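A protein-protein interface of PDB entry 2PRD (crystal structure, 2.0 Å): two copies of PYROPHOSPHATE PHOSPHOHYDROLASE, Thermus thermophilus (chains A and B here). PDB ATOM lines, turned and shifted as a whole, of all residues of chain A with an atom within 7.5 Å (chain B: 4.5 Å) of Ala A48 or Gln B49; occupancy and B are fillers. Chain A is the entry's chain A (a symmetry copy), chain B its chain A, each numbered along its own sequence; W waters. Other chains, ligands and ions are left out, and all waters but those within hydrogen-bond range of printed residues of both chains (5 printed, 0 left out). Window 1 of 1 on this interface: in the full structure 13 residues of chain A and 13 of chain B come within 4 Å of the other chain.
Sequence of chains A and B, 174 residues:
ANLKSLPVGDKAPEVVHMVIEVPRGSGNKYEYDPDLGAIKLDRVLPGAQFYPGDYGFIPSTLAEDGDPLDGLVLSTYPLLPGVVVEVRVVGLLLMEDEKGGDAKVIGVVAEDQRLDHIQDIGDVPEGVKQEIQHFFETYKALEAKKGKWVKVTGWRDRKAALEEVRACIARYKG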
ATOM      1  N   LEU A  45     -16.855 -17.682  14.174  1.00  0.00           N
ATOM      2  CA  LEU A  45     -15.858 -17.673  13.076  1.00  0.00           C
ATOM      3  C   LEU A  45     -14.498 -17.336  13.697  1.00  0.00           C
ATOM      4  O   LEU A  45     -14.441 -16.391  14.476  1.00  0.00           O
ATOM      5  CB  LEU A  45     -16.267 -16.649  12.036  1.00  0.00           C
ATOM      6  CG  LEU A  45     -17.578 -16.725  11.300  1.00  0.00           C
ATOM      7  CD1 LEU A  45     -17.671 -15.534  10.326  1.00  0.00           C
ATOM      8  CD2 LEU A  45     -17.725 -18.042  10.521  1.00  0.00           C
ATOM      9  N   PRO A  46     -13.461 -18.093  13.304  1.00  0.00           N
ATOM     10  CA  PRO A  46     -12.146 -17.897  13.863  1.00  0.00           C
ATOM     11  C   PRO A  46     -11.373 -16.675  13.397  1.00  0.00           C
ATOM     12  O   PRO A  46     -10.433 -16.282  14.107  1.00  0.00           O
ATOM     13  CB  PRO A  46     -11.468 -19.227  13.601  1.00  0.00           C
ATOM     14  CG  PRO A  46     -12.126 -19.726  12.318  1.00  0.00           C
ATOM     15  CD  PRO A  46     -13.559 -19.254  12.397  1.00  0.00           C
ATOM     16  N   GLY A  47     -11.758 -16.096  12.267  1.00  0.00           N
ATOM     17  CA  GLY A  47     -11.041 -14.941  11.735  1.00  0.00           C
ATOM     18  C   GLY A  47     -11.761 -13.659  12.011  1.00  0.00           C
ATOM     19  O   GLY A  47     -12.906 -13.764  12.450  1.00  0.00           O
ATOM     20  N   ALA A  48     -11.084 -12.526  11.753  1.00  0.00           N
ATOM     21  CA  ALA A  48     -11.812 -11.256  12.063  1.00  0.00           C
ATOM     22  C   ALA A  48     -12.727 -10.948  10.907  1.00  0.00           C
ATOM     23  O   ALA A  48     -12.444 -10.041  10.096  1.00  0.00           O
ATOM     24  CB  ALA A  48     -10.681 -10.215  12.239  1.00  0.00           C
ATOM     25  N   GLN A  49     -13.813 -11.706  10.787  1.00  0.00           N
ATOM     26  CA  GLN A  49     -14.817 -11.603   9.768  1.00  0.00           C
ATOM     27  C   GLN A  49     -16.233 -11.665  10.281  1.00  0.00           C
ATOM     28  O   GLN A  49     -16.511 -12.015  11.430  1.00  0.00           O
ATOM     29  CB  GLN A  49     -14.701 -12.829   8.760  1.00  0.00           C
ATOM     30  CG  GLN A  49     -13.264 -12.891   8.265  1.00  0.00           C
ATOM     31  CD  GLN A  49     -12.967 -14.115   7.432  1.00  0.00           C
ATOM     32  OE1 GLN A  49     -13.101 -14.093   6.208  1.00  0.00           O
ATOM     33  NE2 GLN A  49     -12.541 -15.176   8.104  1.00  0.00           N
ATOM     34  N   PHE A  50     -17.125 -11.341   9.342  1.00  0.00           N
ATOM     35  CA  PHE A  50     -18.582 -11.325   9.576  1.00  0.00           C
ATOM     36  C   PHE A  50     -19.303 -11.667   8.283  1.00  0.00           C
ATOM     37  O   PHE A  50     -18.727 -11.442   7.221  1.00  0.00           O
ATOM     38  CB  PHE A  50     -19.002  -9.962  10.155  1.00  0.00           C
ATOM     39  CG  PHE A  50     -18.681  -8.786   9.296  1.00  0.00           C
ATOM     40  CD1 PHE A  50     -19.447  -8.540   8.164  1.00  0.00           C
ATOM     41  CD2 PHE A  50     -17.634  -7.942   9.616  1.00  0.00           C
ATOM     42  CE1 PHE A  50     -19.185  -7.451   7.370  1.00  0.00           C
ATOM     43  CE2 PHE A  50     -17.369  -6.851   8.816  1.00  0.00           C
ATOM     44  CZ  PHE A  50     -18.103  -6.632   7.671  1.00  0.00           C
ATOM     45  N   GLU A 131     -16.828  -9.147  -2.451  1.00  0.00           N
ATOM     46  CA  GLU A 131     -16.807  -9.238  -0.991  1.00  0.00           C
ATOM     47  C   GLU A 131     -17.370 -10.589  -0.587  1.00  0.00           C
ATOM     48  O   GLU A 131     -16.794 -11.294   0.260  1.00  0.00           O
ATOM     49  CB  GLU A 131     -17.571  -8.062  -0.348  1.00  0.00           C
ATOM     50  CG  GLU A 131     -17.425  -8.059   1.191  1.00  0.00           C
ATOM     51  CD  GLU A 131     -18.365  -7.020   1.812  1.00  0.00           C
ATOM     52  OE1 GLU A 131     -19.347  -6.703   1.131  1.00  0.00           O
ATOM     53  OE2 GLU A 131     -18.083  -6.479   2.893  1.00  0.00           O
ATOM     54  N   HIS A 134     -15.012 -13.420  -1.665  1.00  0.00           N
ATOM     55  CA  HIS A 134     -13.772 -13.463  -0.825  1.00  0.00           C
ATOM     56  C   HIS A 134     -14.111 -13.982   0.552  1.00  0.00           C
ATOM     57  O   HIS A 134     -13.305 -14.632   1.232  1.00  0.00           O
ATOM     58  CB  HIS A 134     -13.059 -12.131  -0.915  1.00  0.00           C
ATOM     59  CG  HIS A 134     -11.948 -11.890   0.065  1.00  0.00           C
ATOM     60  ND1 HIS A 134     -12.199 -11.307   1.297  1.00  0.00           N
ATOM     61  CD2 HIS A 134     -10.641 -12.115   0.077  1.00  0.00           C
ATOM     62  CE1 HIS A 134     -11.090 -11.196   1.986  1.00  0.00           C
ATOM     63  NE2 HIS A 134     -10.108 -11.712   1.251  1.00  0.00           N
ATOM     64  N   PHE A 135     -15.349 -13.787   1.014  1.00  0.00           N
ATOM     65  CA  PHE A 135     -15.750 -14.268   2.349  1.00  0.00           C
ATOM     66  C   PHE A 135     -15.726 -15.773   2.403  1.00  0.00           C
ATOM     67  O   PHE A 135     -15.074 -16.415   3.257  1.00  0.00           O
ATOM     68  CB  PHE A 135     -17.106 -13.692   2.785  1.00  0.00           C
ATOM     69  CG  PHE A 135     -17.672 -14.376   4.007  1.00  0.00           C
ATOM     70  CD1 PHE A 135     -17.298 -14.012   5.268  1.00  0.00           C
ATOM     71  CD2 PHE A 135     -18.589 -15.399   3.864  1.00  0.00           C
ATOM     72  CE1 PHE A 135     -17.839 -14.657   6.377  1.00  0.00           C
ATOM     73  CE2 PHE A 135     -19.128 -16.068   4.932  1.00  0.00           C
ATOM     74  CZ  PHE A 135     -18.767 -15.685   6.216  1.00  0.00           C
ATOM     75  N   THR A 138     -12.213 -17.452   2.354  1.00  0.00           N
ATOM     76  CA  THR A 138     -11.252 -17.336   3.447  1.00  0.00           C
ATOM     77  C   THR A 138     -11.833 -17.673   4.802  1.00  0.00           C
ATOM     78  O   THR A 138     -11.046 -17.893   5.749  1.00  0.00           O
ATOM     79  CB  THR A 138     -10.711 -15.885   3.522  1.00  0.00           C
ATOM     80  OG1 THR A 138     -11.828 -14.970   3.624  1.00  0.00           O
ATOM     81  CG2 THR A 138      -9.937 -15.454   2.290  1.00  0.00           C
ATOM     82  N   LEU A 142      -9.023 -20.905   8.664  1.00  0.00           N
ATOM     83  CA  LEU A 142      -8.486 -21.281   9.975  1.00  0.00           C
ATOM     84  C   LEU A 142      -9.029 -22.599  10.517  1.00  0.00           C
ATOM     85  O   LEU A 142      -8.686 -23.070  11.616  1.00  0.00           O
ATOM     86  CB  LEU A 142      -8.716 -20.128  10.978  1.00  0.00           C
ATOM     87  CG  LEU A 142      -7.977 -18.848  10.555  1.00  0.00           C
ATOM     88  CD1 LEU A 142      -8.269 -17.651  11.379  1.00  0.00           C
ATOM     89  CD2 LEU A 142      -6.464 -19.132  10.684  1.00  0.00           C
ATOM     90  N   GLY B  27     -14.041  -1.262   9.844  1.00  0.00           N
ATOM     91  CA  GLY B  27     -13.725  -1.535   8.443  1.00  0.00           C
ATOM     92  C   GLY B  27     -13.378  -0.241   7.723  1.00  0.00           C
ATOM     93  O   GLY B  27     -13.074  -0.236   6.519  1.00  0.00           O
ATOM     94  N   LEU B  45     -12.082  -1.029   3.804  1.00  0.00           N
ATOM     95  CA  LEU B  45     -11.578  -2.376   3.443  1.00  0.00           C
ATOM     96  C   LEU B  45     -12.606  -3.010   2.500  1.00  0.00           C
ATOM     97  O   LEU B  45     -13.789  -2.951   2.814  1.00  0.00           O
ATOM     98  CB  LEU B  45     -11.397  -3.198   4.704  1.00  0.00           C
ATOM     99  CG  LEU B  45     -10.472  -2.778   5.814  1.00  0.00           C
ATOM    100  CD1 LEU B  45     -10.531  -3.833   6.937  1.00  0.00           C
ATOM    101  CD2 LEU B  45      -9.022  -2.622   5.328  1.00  0.00           C
ATOM    102  N   GLY B  47     -13.138  -6.218   1.784  1.00  0.00           N
ATOM    103  CA  GLY B  47     -13.706  -7.506   2.171  1.00  0.00           C
ATOM    104  C   GLY B  47     -14.542  -7.402   3.407  1.00  0.00           C
ATOM    105  O   GLY B  47     -14.477  -6.334   4.017  1.00  0.00           O
ATOM    106  N   ALA B  48     -15.279  -8.481   3.724  1.00  0.00           N
ATOM    107  CA  ALA B  48     -16.129  -8.344   4.948  1.00  0.00           C
ATOM    108  C   ALA B  48     -15.263  -8.608   6.150  1.00  0.00           C
ATOM    109  O   ALA B  48     -15.354  -9.686   6.775  1.00  0.00           O
ATOM    110  CB  ALA B  48     -17.237  -9.405   4.749  1.00  0.00           C
ATOM    111  N   GLN B  49     -14.391  -7.659   6.479  1.00  0.00           N
ATOM    112  CA  GLN B  49     -13.464  -7.694   7.572  1.00  0.00           C
ATOM    113  C   GLN B  49     -13.405  -6.420   8.379  1.00  0.00           C
ATOM    114  O   GLN B  49     -13.918  -5.366   7.998  1.00  0.00           O
ATOM    115  CB  GLN B  49     -11.983  -7.892   7.027  1.00  0.00           C
ATOM    116  CG  GLN B  49     -11.979  -9.114   6.123  1.00  0.00           C
ATOM    117  CD  GLN B  49     -10.671  -9.321   5.396  1.00  0.00           C
ATOM    118  OE1 GLN B  49      -9.781 -10.017   5.885  1.00  0.00           O
ATOM    119  NE2 GLN B  49     -10.572  -8.729   4.214  1.00  0.00           N
ATOM    120  N   PHE B  50     -12.710  -6.570   9.508  1.00  0.00           N
ATOM    121  CA  PHE B  50     -12.492  -5.480  10.479  1.00  0.00           C
ATOM    122  C   PHE B  50     -11.157  -5.686  11.177  1.00  0.00           C
ATOM    123  O   PHE B  50     -10.706  -6.826  11.239  1.00  0.00           O
ATOM    124  CB  PHE B  50     -13.677  -5.412  11.460  1.00  0.00           C
ATOM    125  CG  PHE B  50     -13.920  -6.658  12.243  1.00  0.00           C
ATOM    126  CD1 PHE B  50     -13.069  -6.978  13.294  1.00  0.00           C
ATOM    127  CD2 PHE B  50     -14.979  -7.492  11.934  1.00  0.00           C
ATOM    128  CE1 PHE B  50     -13.285  -8.109  14.043  1.00  0.00           C
ATOM    129  CE2 PHE B  50     -15.193  -8.627  12.685  1.00  0.00           C
ATOM    130  CZ  PHE B  50     -14.326  -8.966  13.699  1.00  0.00           C
ATOM    131  N   PRO B  52      -8.596  -6.484  13.816  1.00  0.00           N
ATOM    132  CA  PRO B  52      -8.653  -7.372  14.975  1.00  0.00           C
ATOM    133  C   PRO B  52      -8.260  -6.698  16.259  1.00  0.00           C
ATOM    134  O   PRO B  52      -8.425  -7.242  17.378  1.00  0.00           O
ATOM    135  CB  PRO B  52      -7.836  -8.565  14.465  1.00  0.00           C
ATOM    136  CG  PRO B  52      -6.693  -7.805  13.776  1.00  0.00           C
ATOM    137  CD  PRO B  52      -7.472  -6.817  12.912  1.00  0.00           C
ATOM    138  N   GLU B 131      -5.851 -15.144  14.347  1.00  0.00           N
ATOM    139  CA  GLU B 131      -6.834 -14.196  13.822  1.00  0.00           C
ATOM    140  C   GLU B 131      -6.089 -13.008  13.240  1.00  0.00           C
ATOM    141  O   GLU B 131      -6.385 -12.551  12.122  1.00  0.00           O
ATOM    142  CB  GLU B 131      -7.849 -13.786  14.907  1.00  0.00           C
ATOM    143  CG  GLU B 131      -8.982 -12.908  14.328  1.00  0.00           C
ATOM    144  CD  GLU B 131      -9.845 -12.339  15.460  1.00  0.00           C
ATOM    145  OE1 GLU B 131      -9.303 -12.264  16.567  1.00  0.00           O
ATOM    146  OE2 GLU B 131     -11.041 -12.066  15.266  1.00  0.00           O
ATOM    147  N   PHE B 135      -5.688 -11.969   9.286  1.00  0.00           N
ATOM    148  CA  PHE B 135      -6.214 -10.662   8.852  1.00  0.00           C
ATOM    149  C   PHE B 135      -5.279 -10.012   7.867  1.00  0.00           C
ATOM    150  O   PHE B 135      -5.642  -9.626   6.732  1.00  0.00           O
ATOM    151  CB  PHE B 135      -6.532  -9.744  10.043  1.00  0.00           C
ATOM    152  CG  PHE B 135      -6.801  -8.316   9.632  1.00  0.00           C
ATOM    153  CD1 PHE B 135      -8.034  -7.915   9.205  1.00  0.00           C
ATOM    154  CD2 PHE B 135      -5.786  -7.381   9.680  1.00  0.00           C
ATOM    155  CE1 PHE B 135      -8.254  -6.590   8.837  1.00  0.00           C
ATOM    156  CE2 PHE B 135      -5.963  -6.074   9.308  1.00  0.00           C
ATOM    157  CZ  PHE B 135      -7.220  -5.657   8.895  1.00  0.00           C
ATOM    158  N   THR B 138      -5.101 -11.625   4.326  1.00  0.00           N
ATOM    159  CA  THR B 138      -6.211 -11.607   3.379  1.00  0.00           C
ATOM    160  C   THR B 138      -6.795 -10.231   3.157  1.00  0.00           C
ATOM    161  O   THR B 138      -7.536 -10.052   2.166  1.00  0.00           O
ATOM    162  CB  THR B 138      -7.354 -12.521   3.890  1.00  0.00           C
ATOM    163  OG1 THR B 138      -7.720 -12.114   5.230  1.00  0.00           O
ATOM    164  CG2 THR B 138      -6.970 -13.985   3.996  1.00  0.00           C
ATOM    165  N   TYR B 139      -6.511  -9.288   4.023  1.00  0.00           N
ATOM    166  CA  TYR B 139      -7.168  -7.971   3.942  1.00  0.00           C
ATOM    167  C   TYR B 139      -6.863  -7.130   2.746  1.00  0.00           C
ATOM    168  O   TYR B 139      -7.650  -6.240   2.397  1.00  0.00           O
ATOM    169  CB  TYR B 139      -7.052  -7.209   5.239  1.00  0.00           C
ATOM    170  CG  TYR B 139      -5.875  -6.262   5.417  1.00  0.00           C
ATOM    171  CD1 TYR B 139      -4.585  -6.747   5.398  1.00  0.00           C
ATOM    172  CD2 TYR B 139      -6.048  -4.923   5.679  1.00  0.00           C
ATOM    173  CE1 TYR B 139      -3.478  -5.963   5.620  1.00  0.00           C
ATOM    174  CE2 TYR B 139      -4.960  -4.101   5.905  1.00  0.00           C
ATOM    175  CZ  TYR B 139      -3.690  -4.625   5.868  1.00  0.00           C
ATOM    176  OH  TYR B 139      -2.592  -3.822   6.091  1.00  0.00           O
HETATM  177  O   HOH W   1     -14.365 -11.652   4.939  1.00  0.00           O
HETATM  178  O   HOH W   2      -9.301  -8.403   0.493  1.00  0.00           O
HETATM  179  O   HOH W   3     -14.698 -10.629   2.306  1.00  0.00           O
HETATM  180  O   HOH W   4     -10.128 -11.022   8.720  1.00  0.00           O
HETATM  181  O   HOH W   5      -8.836 -12.900  10.422  1.00  0.00           O
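The backbone carbonyl oxygen (O) of Thr B138 sits at hydrogen-bond distance from a ring nitrogen (NE2) of His A134, at 3.2 Å.
OG1 of Thr A138 sits at hydrogen-bond distance from OE1 of Gln A49.
The backbone carbonyl oxygen of His A134 lies within hydrogen-bond range of the side-chain hydroxyl of Thr A138 (2.8 Å).
The side-chain amide oxygen (OE1) of Gln B49 sits at hydrogen-bond distance from the side-chain hydroxyl (OG1) of Thr B138 (3.0 Å).
Ala A48 touches just these residues of chain B: Gln B49 (3.6 Å), Phe B50 (3.5 Å), Pro B52 (3.97 Å) and Glu B131 (3.3 Å).
Of chain A, only Ala A48 (3.6 Å), Phe A50 (3.8 Å) and His A134 (3.4 Å) come within 4 Å of Gln B49.
Of the printed residues of chain B, His A134 touches Gln B49 and Thr B138.
Printed residues of chain A within 4 Å of Glu B131: Pro A46 (3.7 Å), Gly A47 (3.7 Å) and Ala A48 (3.3 Å).
Printed residues of chain A within 4 Å of Pro B52: Ala A48 (3.97 Å).
Printed residues of chain B within 4 Å of Phe A50: Ala B48, Gln B49 and Phe B50.
The nearest residue of chain B that does not touch Ala A48 is Ala B48 (4.4 Å).
Water W3 lies within hydrogen-bond range of the backbone NH (N) of Ala B48 (2.6 Å), a ring nitrogen (ND1) of His A134 (2.8 Å), the backbone carbonyl oxygen (O) of Glu A131 (3.0 Å) and the backbone NH (N) of Phe A135 (3.5 Å).
Water W5 lies within hydrogen-bond range of the backbone NH (N) of Ala A48 (2.6 Å), the backbone carbonyl oxygen (O) of Glu B131 (3.0 Å) and the backbone NH (N) of Phe B135 (3.5 Å).
Water W1 bridges O of Ala B48 and OE1 of Gln A49.
Water W4 lies within hydrogen-bond range of O of Ala A48 (2.9 Å) and OE1 of Gln B49 (3.0 Å).
Water W2 lies within hydrogen-bond range of the backbone carbonyl oxygen (O) of Thr B138, the backbone carbonyl oxygen (O) of Tyr B139 and a ring nitrogen (NE2) of His A134.
Among the printed residues, merely in contact across the chains: Pro A46 with Glu B131, Gly A47 with Glu B131, Ala A48 with Gln B49, Ala A48 with Phe B50, Ala A48 with Pro B52, Ala A48 with Glu B131, Gln A49 with Ala B48, Gln A49 with Phe B50, Phe A50 with Ala B48, Phe A50 with Gln B49, Phe A50 with Phe B50, Glu A131 with Gly B47, Glu A131 with Ala B48, His A134 with Gln B49 and Thr A138 with Thr B138.
Gly A47 touches Glu B131, and with the chains exchanged Glu A131 touches Gly B47.
Ala A48 touches Phe B50, and with the chains exchanged Phe A50 touches Ala B48.
Gln A49 touches Phe B50, and with the chains exchanged Phe A50 touches Gln B49.
Phe B50 touches its own counterpart, Phe A50.
8 positions are printed for both chains.
Of the 11 printed residues of chain B, 7 touch a printed residue of chain A.
Hydrophobic or aromatic side chains of chain B within 4 Å of the printed part of chain A: Ala B48, Phe B50 and Pro B52.
Of the 11 printed residues of chain A, 8 touch a printed residue of chain B.
Hydrophobic or aromatic side chains of chain A that line the printed part of chain B: Ala A48, Phe A50 and His A134.
Among the printed residues, 16 pairs touch across the chains.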
